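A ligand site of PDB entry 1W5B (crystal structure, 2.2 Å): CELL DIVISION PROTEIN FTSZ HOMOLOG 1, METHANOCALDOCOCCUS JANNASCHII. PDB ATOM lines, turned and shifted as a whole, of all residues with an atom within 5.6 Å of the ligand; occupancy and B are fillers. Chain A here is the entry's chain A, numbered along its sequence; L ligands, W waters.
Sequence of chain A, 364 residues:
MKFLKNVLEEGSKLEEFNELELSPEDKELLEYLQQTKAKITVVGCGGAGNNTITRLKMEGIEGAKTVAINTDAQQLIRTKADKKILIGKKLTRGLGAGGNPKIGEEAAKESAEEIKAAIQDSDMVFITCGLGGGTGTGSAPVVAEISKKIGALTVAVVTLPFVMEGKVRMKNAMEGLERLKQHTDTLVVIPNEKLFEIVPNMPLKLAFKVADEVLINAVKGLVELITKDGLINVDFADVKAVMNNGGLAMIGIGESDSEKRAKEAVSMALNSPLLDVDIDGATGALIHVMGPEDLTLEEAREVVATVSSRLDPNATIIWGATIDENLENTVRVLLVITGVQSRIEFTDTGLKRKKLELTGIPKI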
ATOM      1  N   CYS A  45      11.827  -1.878  19.900  1.00  0.00           N
ATOM      2  CA  CYS A  45      12.355  -3.204  20.186  1.00  0.00           C
ATOM      3  C   CYS A  45      11.623  -3.856  21.349  1.00  0.00           C
ATOM      4  O   CYS A  45      11.393  -3.211  22.370  1.00  0.00           O
ATOM      5  CB  CYS A  45      13.839  -3.116  20.541  1.00  0.00           C
ATOM      6  SG  CYS A  45      14.799  -2.019  19.481  1.00  0.00           S
ATOM      7  N   GLY A  46      11.292  -5.136  21.214  1.00  0.00           N
ATOM      8  CA  GLY A  46      10.574  -5.834  22.281  1.00  0.00           C
ATOM      9  C   GLY A  46       9.094  -5.489  22.351  1.00  0.00           C
ATOM     10  O   GLY A  46       8.598  -4.670  21.575  1.00  0.00           O
ATOM     11  N   GLY A  47       8.395  -6.128  23.279  1.00  0.00           N
ATOM     12  CA  GLY A  47       6.968  -5.901  23.436  1.00  0.00           C
ATOM     13  C   GLY A  47       6.556  -4.453  23.711  1.00  0.00           C
ATOM     14  O   GLY A  47       5.687  -3.913  23.025  1.00  0.00           O
ATOM     15  N   ALA A  48       7.147  -3.833  24.722  1.00  0.00           N
ATOM     16  CA  ALA A  48       6.815  -2.433  25.029  1.00  0.00           C
ATOM     17  C   ALA A  48       7.169  -1.571  23.814  1.00  0.00           C
ATOM     18  O   ALA A  48       6.431  -0.657  23.465  1.00  0.00           O
ATOM     19  CB  ALA A  48       7.588  -1.949  26.265  1.00  0.00           C
ATOM     20  N   GLY A  49       8.300  -1.874  23.190  1.00  0.00           N
ATOM     21  CA  GLY A  49       8.703  -1.111  22.024  1.00  0.00           C
ATOM     22  C   GLY A  49       7.739  -1.301  20.866  1.00  0.00           C
ATOM     23  O   GLY A  49       7.400  -0.331  20.169  1.00  0.00           O
ATOM     24  N   ASN A  51       4.591  -2.145  21.112  1.00  0.00           N
ATOM     25  CA  ASN A  51       3.326  -1.522  21.495  1.00  0.00           C
ATOM     26  C   ASN A  51       3.370  -0.037  21.162  1.00  0.00           C
ATOM     27  O   ASN A  51       2.408   0.530  20.648  1.00  0.00           O
ATOM     28  CB  ASN A  51       3.058  -1.733  22.993  1.00  0.00           C
ATOM     29  CG  ASN A  51       1.716  -1.170  23.439  1.00  0.00           C
ATOM     30  OD1 ASN A  51       0.679  -1.476  22.856  1.00  0.00           O
ATOM     31  ND2 ASN A  51       1.742  -0.345  24.475  1.00  0.00           N
ATOM     32  N   ASN A  70      11.503  -7.861  17.202  1.00  0.00           N
ATOM     33  CA  ASN A  70      11.234  -8.644  18.379  1.00  0.00           C
ATOM     34  C   ASN A  70      11.695 -10.061  18.107  1.00  0.00           C
ATOM     35  O   ASN A  70      11.886 -10.462  16.959  1.00  0.00           O
ATOM     36  CB  ASN A  70       9.733  -8.609  18.668  1.00  0.00           C
ATOM     37  CG  ASN A  70       9.396  -8.828  20.143  1.00  0.00           C
ATOM     38  OD1 ASN A  70       8.364  -8.344  20.627  1.00  0.00           O
ATOM     39  ND2 ASN A  70      10.232  -9.573  20.855  1.00  0.00           N
ATOM     40  N   THR A  71      11.916 -10.800  19.193  1.00  0.00           N
ATOM     41  CA  THR A  71      12.282 -12.191  19.118  1.00  0.00           C
ATOM     42  C   THR A  71      10.937 -12.944  19.105  1.00  0.00           C
ATOM     43  O   THR A  71      10.762 -13.935  18.388  1.00  0.00           O
ATOM     44  CB  THR A  71      13.093 -12.586  20.359  1.00  0.00           C
ATOM     45  OG1 THR A  71      12.441 -12.068  21.519  1.00  0.00           O
ATOM     46  CG2 THR A  71      14.506 -12.018  20.288  1.00  0.00           C
ATOM     47  N   GLN A  75       4.076 -11.431  19.501  1.00  0.00           N
ATOM     48  CA  GLN A  75       3.926 -10.010  19.764  1.00  0.00           C
ATOM     49  C   GLN A  75       4.109  -9.227  18.468  1.00  0.00           C
ATOM     50  O   GLN A  75       3.369  -8.277  18.201  1.00  0.00           O
ATOM     51  CB  GLN A  75       4.959  -9.521  20.798  1.00  0.00           C
ATOM     52  CG  GLN A  75       4.775 -10.088  22.195  1.00  0.00           C
ATOM     53  CD  GLN A  75       5.732  -9.478  23.209  1.00  0.00           C
ATOM     54  OE1 GLN A  75       6.855  -9.102  22.859  1.00  0.00           O
ATOM     55  NE2 GLN A  75       5.300  -9.384  24.462  1.00  0.00           N
ATOM     56  N   GLY A  96      10.007 -15.370  22.805  1.00  0.00           N
ATOM     57  CA  GLY A  96      10.568 -14.234  23.531  1.00  0.00           C
ATOM     58  C   GLY A  96      11.891 -14.613  24.156  1.00  0.00           C
ATOM     59  O   GLY A  96      12.339 -15.763  24.045  1.00  0.00           O
ATOM     60  N   ALA A  97      12.527 -13.649  24.837  1.00  0.00           N
ATOM     61  CA  ALA A  97      13.817 -13.887  25.473  1.00  0.00           C
ATOM     62  C   ALA A  97      13.699 -14.297  26.944  1.00  0.00           C
ATOM     63  O   ALA A  97      14.710 -14.452  27.630  1.00  0.00           O
ATOM     64  CB  ALA A  97      14.688 -12.638  25.355  1.00  0.00           C
ATOM     65  N   GLY A  98      12.469 -14.456  27.421  1.00  0.00           N
ATOM     66  CA  GLY A  98      12.268 -14.854  28.802  1.00  0.00           C
ATOM     67  C   GLY A  98      12.980 -13.995  29.829  1.00  0.00           C
ATOM     68  O   GLY A  98      13.378 -14.489  30.880  1.00  0.00           O
ATOM     69  N   GLY A  99      13.163 -12.717  29.522  1.00  0.00           N
ATOM     70  CA  GLY A  99      13.824 -11.795  30.441  1.00  0.00           C
ATOM     71  C   GLY A  99      15.350 -11.775  30.432  1.00  0.00           C
ATOM     72  O   GLY A  99      15.961 -11.061  31.226  1.00  0.00           O
ATOM     73  N   ASN A 100      15.965 -12.553  29.541  1.00  0.00           N
ATOM     74  CA  ASN A 100      17.418 -12.632  29.457  1.00  0.00           C
ATOM     75  C   ASN A 100      17.988 -11.631  28.444  1.00  0.00           C
ATOM     76  O   ASN A 100      17.927 -11.860  27.229  1.00  0.00           O
ATOM     77  CB  ASN A 100      17.827 -14.044  29.049  1.00  0.00           C
ATOM     78  CG  ASN A 100      19.297 -14.312  29.258  1.00  0.00           C
ATOM     79  OD1 ASN A 100      20.147 -13.472  28.943  1.00  0.00           O
ATOM     80  ND2 ASN A 100      19.622 -15.494  29.768  1.00  0.00           N
ATOM     81  N   GLY A 130      11.124  -0.627  26.379  1.00  0.00           N
ATOM     82  CA  GLY A 130      11.028  -0.589  27.821  1.00  0.00           C
ATOM     83  C   GLY A 130      12.197  -1.430  28.313  1.00  0.00           C
ATOM     84  O   GLY A 130      12.308  -2.604  27.956  1.00  0.00           O
ATOM     85  N   LEU A 131      13.093  -0.840  29.100  1.00  0.00           N
ATOM     86  CA  LEU A 131      14.240  -1.590  29.600  1.00  0.00           C
ATOM     87  C   LEU A 131      13.811  -2.480  30.767  1.00  0.00           C
ATOM     88  O   LEU A 131      12.933  -2.095  31.546  1.00  0.00           O
ATOM     89  CB  LEU A 131      15.349  -0.638  30.043  1.00  0.00           C
ATOM     90  CG  LEU A 131      15.925   0.284  28.958  1.00  0.00           C
ATOM     91  CD1 LEU A 131      16.952   1.205  29.583  1.00  0.00           C
ATOM     92  CD2 LEU A 131      16.572  -0.542  27.850  1.00  0.00           C
ATOM     93  N   GLY A 132      14.405  -3.668  30.871  1.00  0.00           N
ATOM     94  CA  GLY A 132      14.036  -4.578  31.936  1.00  0.00           C
ATOM     95  C   GLY A 132      13.790  -6.000  31.460  1.00  0.00           C
ATOM     96  O   GLY A 132      13.976  -6.956  32.201  1.00  0.00           O
ATOM     97  N   GLY A 133      13.353  -6.146  30.215  1.00  0.00           N
ATOM     98  CA  GLY A 133      13.097  -7.469  29.671  1.00  0.00           C
ATOM     99  C   GLY A 133      14.348  -7.973  28.968  1.00  0.00           C
ATOM    100  O   GLY A 133      15.388  -7.341  29.041  1.00  0.00           O
ATOM    101  N   GLY A 134      14.243  -9.102  28.278  1.00  0.00           N
ATOM    102  CA  GLY A 134      15.413  -9.617  27.592  1.00  0.00           C
ATOM    103  C   GLY A 134      15.651  -9.081  26.190  1.00  0.00           C
ATOM    104  O   GLY A 134      16.790  -8.895  25.782  1.00  0.00           O
ATOM    105  N   THR A 135      14.581  -8.817  25.445  1.00  0.00           N
ATOM    106  CA  THR A 135      14.731  -8.339  24.077  1.00  0.00           C
ATOM    107  C   THR A 135      15.086  -6.868  23.933  1.00  0.00           C
ATOM    108  O   THR A 135      16.117  -6.531  23.364  1.00  0.00           O
ATOM    109  CB  THR A 135      13.459  -8.631  23.258  1.00  0.00           C
ATOM    110  OG1 THR A 135      13.289 -10.056  23.156  1.00  0.00           O
ATOM    111  CG2 THR A 135      13.568  -8.050  21.858  1.00  0.00           C
ATOM    112  N   GLY A 136      14.223  -5.985  24.445  1.00  0.00           N
ATOM    113  CA  GLY A 136      14.491  -4.563  24.355  1.00  0.00           C
ATOM    114  C   GLY A 136      15.828  -4.211  24.968  1.00  0.00           C
ATOM    115  O   GLY A 136      16.670  -3.559  24.344  1.00  0.00           O
ATOM    116  N   THR A 137      16.036  -4.651  26.206  1.00  0.00           N
ATOM    117  CA  THR A 137      17.281  -4.370  26.925  1.00  0.00           C
ATOM    118  C   THR A 137      18.544  -4.811  26.165  1.00  0.00           C
ATOM    119  O   THR A 137      19.511  -4.051  26.078  1.00  0.00           O
ATOM    120  CB  THR A 137      17.270  -5.058  28.287  1.00  0.00           C
ATOM    121  OG1 THR A 137      16.116  -4.640  29.025  1.00  0.00           O
ATOM    122  CG2 THR A 137      18.529  -4.697  29.070  1.00  0.00           C
ATOM    123  N   THR A 159      12.320   3.615  28.805  1.00  0.00           N
ATOM    124  CA  THR A 159      11.761   3.723  30.147  1.00  0.00           C
ATOM    125  C   THR A 159      12.450   2.727  31.062  1.00  0.00           C
ATOM    126  O   THR A 159      12.938   1.694  30.618  1.00  0.00           O
ATOM    127  CB  THR A 159      10.269   3.373  30.184  1.00  0.00           C
ATOM    128  OG1 THR A 159      10.097   2.004  29.784  1.00  0.00           O
ATOM    129  CG2 THR A 159       9.470   4.283  29.274  1.00  0.00           C
ATOM    130  N   LEU A 160      12.496   3.070  32.344  1.00  0.00           N
ATOM    131  CA  LEU A 160      13.072   2.195  33.371  1.00  0.00           C
ATOM    132  C   LEU A 160      11.828   1.576  33.990  1.00  0.00           C
ATOM    133  O   LEU A 160      10.763   2.197  33.997  1.00  0.00           O
ATOM    134  CB  LEU A 160      13.856   3.032  34.403  1.00  0.00           C
ATOM    135  CG  LEU A 160      15.394   3.142  34.296  1.00  0.00           C
ATOM    136  CD1 LEU A 160      15.902   2.823  32.899  1.00  0.00           C
ATOM    137  CD2 LEU A 160      15.812   4.526  34.715  1.00  0.00           C
ATOM    138  N   PRO A 161      11.921   0.341  34.510  1.00  0.00           N
ATOM    139  CA  PRO A 161      10.762  -0.319  35.101  1.00  0.00           C
ATOM    140  C   PRO A 161      10.264   0.231  36.431  1.00  0.00           C
ATOM    141  O   PRO A 161      10.986   0.955  37.125  1.00  0.00           O
ATOM    142  CB  PRO A 161      11.234  -1.767  35.218  1.00  0.00           C
ATOM    143  CG  PRO A 161      12.687  -1.592  35.564  1.00  0.00           C
ATOM    144  CD  PRO A 161      13.125  -0.507  34.590  1.00  0.00           C
ATOM    145  N   PHE A 162       9.026  -0.112  36.768  1.00  0.00           N
ATOM    146  CA  PHE A 162       8.401   0.302  38.024  1.00  0.00           C
ATOM    147  C   PHE A 162       9.038  -0.519  39.120  1.00  0.00           C
ATOM    148  O   PHE A 162       9.457  -1.651  38.893  1.00  0.00           O
ATOM    149  CB  PHE A 162       6.912  -0.012  38.016  1.00  0.00           C
ATOM    150  CG  PHE A 162       6.094   0.852  37.116  1.00  0.00           C
ATOM    151  CD1 PHE A 162       5.725   2.134  37.518  1.00  0.00           C
ATOM    152  CD2 PHE A 162       5.608   0.356  35.921  1.00  0.00           C
ATOM    153  CE1 PHE A 162       4.880   2.909  36.734  1.00  0.00           C
ATOM    154  CE2 PHE A 162       4.763   1.123  35.117  1.00  0.00           C
ATOM    155  CZ  PHE A 162       4.395   2.398  35.531  1.00  0.00           C
ATOM    156  N   GLU A 165       8.231  -4.129  39.850  1.00  0.00           N
ATOM    157  CA  GLU A 165       8.654  -5.178  38.918  1.00  0.00           C
ATOM    158  C   GLU A 165       9.837  -5.997  39.420  1.00  0.00           C
ATOM    159  O   GLU A 165      10.272  -6.944  38.761  1.00  0.00           O
ATOM    160  CB  GLU A 165       8.982  -4.569  37.544  1.00  0.00           C
ATOM    161  CG  GLU A 165       7.773  -3.979  36.810  1.00  0.00           C
ATOM    162  CD  GLU A 165       8.083  -3.583  35.378  1.00  0.00           C
ATOM    163  OE1 GLU A 165       8.397  -4.485  34.569  1.00  0.00           O
ATOM    164  OE2 GLU A 165       7.999  -2.384  35.046  1.00  0.00           O
ATOM    165  N   ARG A 169      14.759  -7.002  37.435  1.00  0.00           N
ATOM    166  CA  ARG A 169      14.364  -6.278  36.230  1.00  0.00           C
ATOM    167  C   ARG A 169      15.014  -4.890  36.153  1.00  0.00           C
ATOM    168  O   ARG A 169      15.376  -4.432  35.067  1.00  0.00           O
ATOM    169  CB  ARG A 169      12.846  -6.176  36.156  1.00  0.00           C
ATOM    170  CG  ARG A 169      12.305  -5.717  34.829  1.00  0.00           C
ATOM    171  CD  ARG A 169      11.011  -6.455  34.494  1.00  0.00           C
ATOM    172  NE  ARG A 169      11.248  -7.794  33.988  1.00  0.00           N
ATOM    173  CZ  ARG A 169      11.005  -8.174  32.727  1.00  0.00           C
ATOM    174  NH1 ARG A 169      10.509  -7.308  31.848  1.00  0.00           N
ATOM    175  NH2 ARG A 169      11.257  -9.427  32.350  1.00  0.00           N
ATOM    176  N   ASN A 192       9.640   5.120  34.825  1.00  0.00           N
ATOM    177  CA  ASN A 192       8.232   4.757  35.031  1.00  0.00           C
ATOM    178  C   ASN A 192       7.748   4.951  36.474  1.00  0.00           C
ATOM    179  O   ASN A 192       6.625   5.376  36.697  1.00  0.00           O
ATOM    180  CB  ASN A 192       7.980   3.320  34.596  1.00  0.00           C
ATOM    181  CG  ASN A 192       7.631   3.210  33.108  1.00  0.00           C
ATOM    182  OD1 ASN A 192       7.605   2.109  32.545  1.00  0.00           O
ATOM    183  ND2 ASN A 192       7.357   4.344  32.473  1.00  0.00           N
ATOM    184  N   PHE A 208       0.718   0.579  33.199  1.00  0.00           N
ATOM    185  CA  PHE A 208       1.337   0.530  31.882  1.00  0.00           C
ATOM    186  C   PHE A 208       0.581   1.317  30.827  1.00  0.00           C
ATOM    187  O   PHE A 208       1.179   1.793  29.864  1.00  0.00           O
ATOM    188  CB  PHE A 208       1.553  -0.928  31.452  1.00  0.00           C
ATOM    189  CG  PHE A 208       2.590  -1.648  32.279  1.00  0.00           C
ATOM    190  CD1 PHE A 208       3.926  -1.267  32.214  1.00  0.00           C
ATOM    191  CD2 PHE A 208       2.234  -2.683  33.144  1.00  0.00           C
ATOM    192  CE1 PHE A 208       4.899  -1.896  32.990  1.00  0.00           C
ATOM    193  CE2 PHE A 208       3.192  -3.325  33.930  1.00  0.00           C
ATOM    194  CZ  PHE A 208       4.534  -2.926  33.859  1.00  0.00           C
ATOM    195  N   ALA A 211       2.067   4.642  31.302  1.00  0.00           N
ATOM    196  CA  ALA A 211       3.439   4.667  30.784  1.00  0.00           C
ATOM    197  C   ALA A 211       3.365   4.766  29.259  1.00  0.00           C
ATOM    198  O   ALA A 211       4.126   5.515  28.635  1.00  0.00           O
ATOM    199  CB  ALA A 211       4.201   3.414  31.214  1.00  0.00           C
ATOM    200  N   ASP A 212       2.433   4.027  28.654  1.00  0.00           N
ATOM    201  CA  ASP A 212       2.240   4.041  27.208  1.00  0.00           C
ATOM    202  C   ASP A 212       2.039   5.473  26.741  1.00  0.00           C
ATOM    203  O   ASP A 212       2.684   5.940  25.794  1.00  0.00           O
ATOM    204  CB  ASP A 212       0.997   3.235  26.810  1.00  0.00           C
ATOM    205  CG  ASP A 212       1.255   1.746  26.766  1.00  0.00           C
ATOM    206  OD1 ASP A 212       2.374   1.342  27.095  1.00  0.00           O
ATOM    207  OD2 ASP A 212       0.335   0.996  26.386  1.00  0.00           O
ATOM    208  N   LEU A 215       5.246   7.512  26.983  1.00  0.00           N
ATOM    209  CA  LEU A 215       6.175   7.113  25.924  1.00  0.00           C
ATOM    210  C   LEU A 215       5.777   7.727  24.591  1.00  0.00           C
ATOM    211  O   LEU A 215       6.589   8.371  23.926  1.00  0.00           O
ATOM    212  CB  LEU A 215       6.228   5.598  25.788  1.00  0.00           C
ATOM    213  CG  LEU A 215       7.435   4.899  26.429  1.00  0.00           C
ATOM    214  CD1 LEU A 215       7.260   3.400  26.281  1.00  0.00           C
ATOM    215  CD2 LEU A 215       8.737   5.361  25.757  1.00  0.00           C
HETATM  216  P1  LIG L   1      11.403 -10.410  26.635  1.00  0.00           P
HETATM  217  O1  LIG L   1      12.172 -10.987  27.843  1.00  0.00           O
HETATM  218  O2  LIG L   1       9.893 -10.694  26.731  1.00  0.00           O
HETATM  219  O3  LIG L   1      11.888 -11.049  25.324  1.00  0.00           O
HETATM  220  O4  LIG L   1      11.752  -8.786  26.600  1.00  0.00           O
HETATM  221  P2  LIG L   1      10.877  -7.504  26.067  1.00  0.00           P
HETATM  222  O5  LIG L   1       9.902  -7.853  25.036  1.00  0.00           O
HETATM  223  O6  LIG L   1      11.916  -6.453  25.732  1.00  0.00           O
HETATM  224  O7  LIG L   1      10.067  -6.989  27.279  1.00  0.00           O
HETATM  225  P3  LIG L   1       8.881  -6.006  27.369  1.00  0.00           P
HETATM  226  O8  LIG L   1       7.596  -6.765  27.443  1.00  0.00           O
HETATM  227  O9  LIG L   1       9.004  -4.941  26.387  1.00  0.00           O
HETATM  228  O10 LIG L   1       9.139  -5.485  28.890  1.00  0.00           O
HETATM  229  C1  LIG L   1      10.236  -4.638  29.241  1.00  0.00           C
HETATM  230  C2  LIG L   1       9.754  -3.559  30.193  1.00  0.00           C
HETATM  231  O11 LIG L   1       8.783  -2.738  29.523  1.00  0.00           O
HETATM  232  C3  LIG L   1       9.035  -4.131  31.420  1.00  0.00           C
HETATM  233  O12 LIG L   1       9.960  -4.391  32.457  1.00  0.00           O
HETATM  234  C4  LIG L   1       8.082  -2.995  31.813  1.00  0.00           C
HETATM  235  O13 LIG L   1       8.804  -2.012  32.551  1.00  0.00           O
HETATM  236  C5  LIG L   1       7.759  -2.367  30.442  1.00  0.00           C
HETATM  237  N1  LIG L   1       6.454  -2.739  29.888  1.00  0.00           N
HETATM  238  C6  LIG L   1       5.959  -4.033  29.697  1.00  0.00           C
HETATM  239  N2  LIG L   1       4.875  -4.084  28.952  1.00  0.00           N
HETATM  240  C7  LIG L   1       4.590  -2.758  28.702  1.00  0.00           C
HETATM  241  C8  LIG L   1       3.566  -2.144  27.931  1.00  0.00           C
HETATM  242  O14 LIG L   1       2.558  -2.674  27.487  1.00  0.00           O
HETATM  243  N3  LIG L   1       3.693  -0.742  27.867  1.00  0.00           N
HETATM  244  C9  LIG L   1       4.687  -0.005  28.489  1.00  0.00           C
HETATM  245  N4  LIG L   1       4.580   1.291  28.470  1.00  0.00           N
HETATM  246  N5  LIG L   1       5.705  -0.562  29.122  1.00  0.00           N
HETATM  247  C10 LIG L   1       5.639  -1.923  29.170  1.00  0.00           C
HETATM  248  O   HOH W   1      13.417  -4.994  27.455  1.00  0.00           O
HETATM  249  O   HOH W   2       7.382   1.644  29.857  1.00  0.00           O
HETATM  250  O   HOH W   3      10.565  -0.095  31.408  1.00  0.00           O
HETATM  251  O   HOH W   4       0.058  -1.270  27.583  1.00  0.00           O
HETATM  252  O   HOH W   5      10.437  -3.043  24.913  1.00  0.00           O
HETATM  253  O   HOH W   6       7.495  -9.224  26.160  1.00  0.00           O
HETATM  254  O   HOH W   7       9.944 -13.622  26.946  1.00  0.00           O
HETATM  255  O   HOH W   8       7.936 -12.583  24.892  1.00  0.00           O
HETATM  256  O   HOH W   9       4.770  -6.285  26.965  1.00  0.00           O
HETATM  257  O   HOH W  10       9.631 -10.453  23.449  1.00  0.00           O
HETATM  258  O   HOH W  11       4.383   0.520  25.013  1.00  0.00           O
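OD1 of Asp 212 lies within hydrogen-bond range of N3 of the ligand (2.6 Å).
N of Gly 99 is in hydrogen-bond range of O1 of the ligand, at 2.6 Å.
The side-chain carboxylate (OE1) of Glu 165 lies within hydrogen-bond range of an oxygen (O12) of the ligand.
The backbone NH of Gly 136 sits at hydrogen-bond distance from an oxygen (O6) of the ligand, at 2.7 Å.
The backbone NH of Ala 97 lies within hydrogen-bond range of an oxygen (O3) of the ligand (2.7 Å).
The backbone NH (N) of Ala 48 lies within hydrogen-bond range of an oxygen (O9) of the ligand (2.7 Å).
The backbone NH of Thr 135 is in hydrogen-bond range of an oxygen (O4) of the ligand (3.1 Å).
OG1 of Thr 135 lies within hydrogen-bond range of O3 of the ligand, at 2.8 Å.
N of Gly 134 is in hydrogen-bond range of O1 of the ligand (2.8 Å).
The backbone NH (N) of Gly 47 lies within hydrogen-bond range of an oxygen (O5) of the ligand.
NH1 of Arg 169 sits at hydrogen-bond distance from O12 of the ligand.
OD2 of Asp 212 sits at hydrogen-bond distance from ND2 of Asn 51, 2.7 Å away.
The side-chain carboxylate of Glu 165 lies within hydrogen-bond range of the backbone NH of Phe 162 (3.0 Å).
The side-chain hydroxyl of Thr 71 lies within hydrogen-bond range of the side-chain hydroxyl of Thr 135 (2.7 Å).
N of Gly 47 lies close to OE1 of Gln 75 (3.4 Å).
NE of Arg 169 lies close to O of Gly 132.
OG1 of Thr 137 lies within hydrogen-bond range of O of Gly 133 (2.8 Å).
N of Leu 131 is in hydrogen-bond range of O of Thr 159, at 3.0 Å.
The side-chain amide oxygen (OD1) of Asn 70 sits close to the side-chain amide oxygen (OE1) of Gln 75 (2.8 Å).
Merely in contact with the ligand: Gly 46, Asn 51, Thr 71, Gln 75, Gly 96, Gly 98, Gly 130, Leu 131, Gly 133, Pro 161, Phe 208 and Ala 211.
Of the 33 residues printed, 22 come within 4 Å of the ligand.
Along chain A the residues within 4 Å of the ligand span positions 46 to 212.
The nearest printed residue that does not touch the ligand is Leu 215 (4.1 Å).
Water W6 bridges an oxygen (O8) of the ligand (2.8 Å) and the side-chain amide nitrogen (NE2) of Gln 75 (2.8 Å).
Water W3 lies within hydrogen-bond range of the side-chain hydroxyl (OG1) of Thr 159, an oxygen (O13) of the ligand, the backbone carbonyl oxygen (O) of Leu 131 and the backbone carbonyl oxygen (O) of Leu 160.
Water W2 lies within hydrogen-bond range of the side-chain amide oxygen (OD1) of Asn 192 (2.7 Å), the side-chain hydroxyl (OG1) of Thr 159 (2.7 Å) and a nitrogen (N5) of the ligand (2.9 Å).
Water W4 lies within hydrogen-bond range of OD2 of Asp 212 (2.6 Å) and O14 of the ligand (2.9 Å).
Water W10 lies within hydrogen-bond range of ND2 of Asn 70 (2.8 Å), O3 of the ligand (3.0 Å) and OE1 of Gln 75 (3.1 Å).
Water W11 lies within hydrogen-bond range of O of Ala 48 (2.8 Å), ND2 of Asn 51 (2.8 Å), OD1 of Asp 212 (3.0 Å) and N3 of the ligand (3.2 Å).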
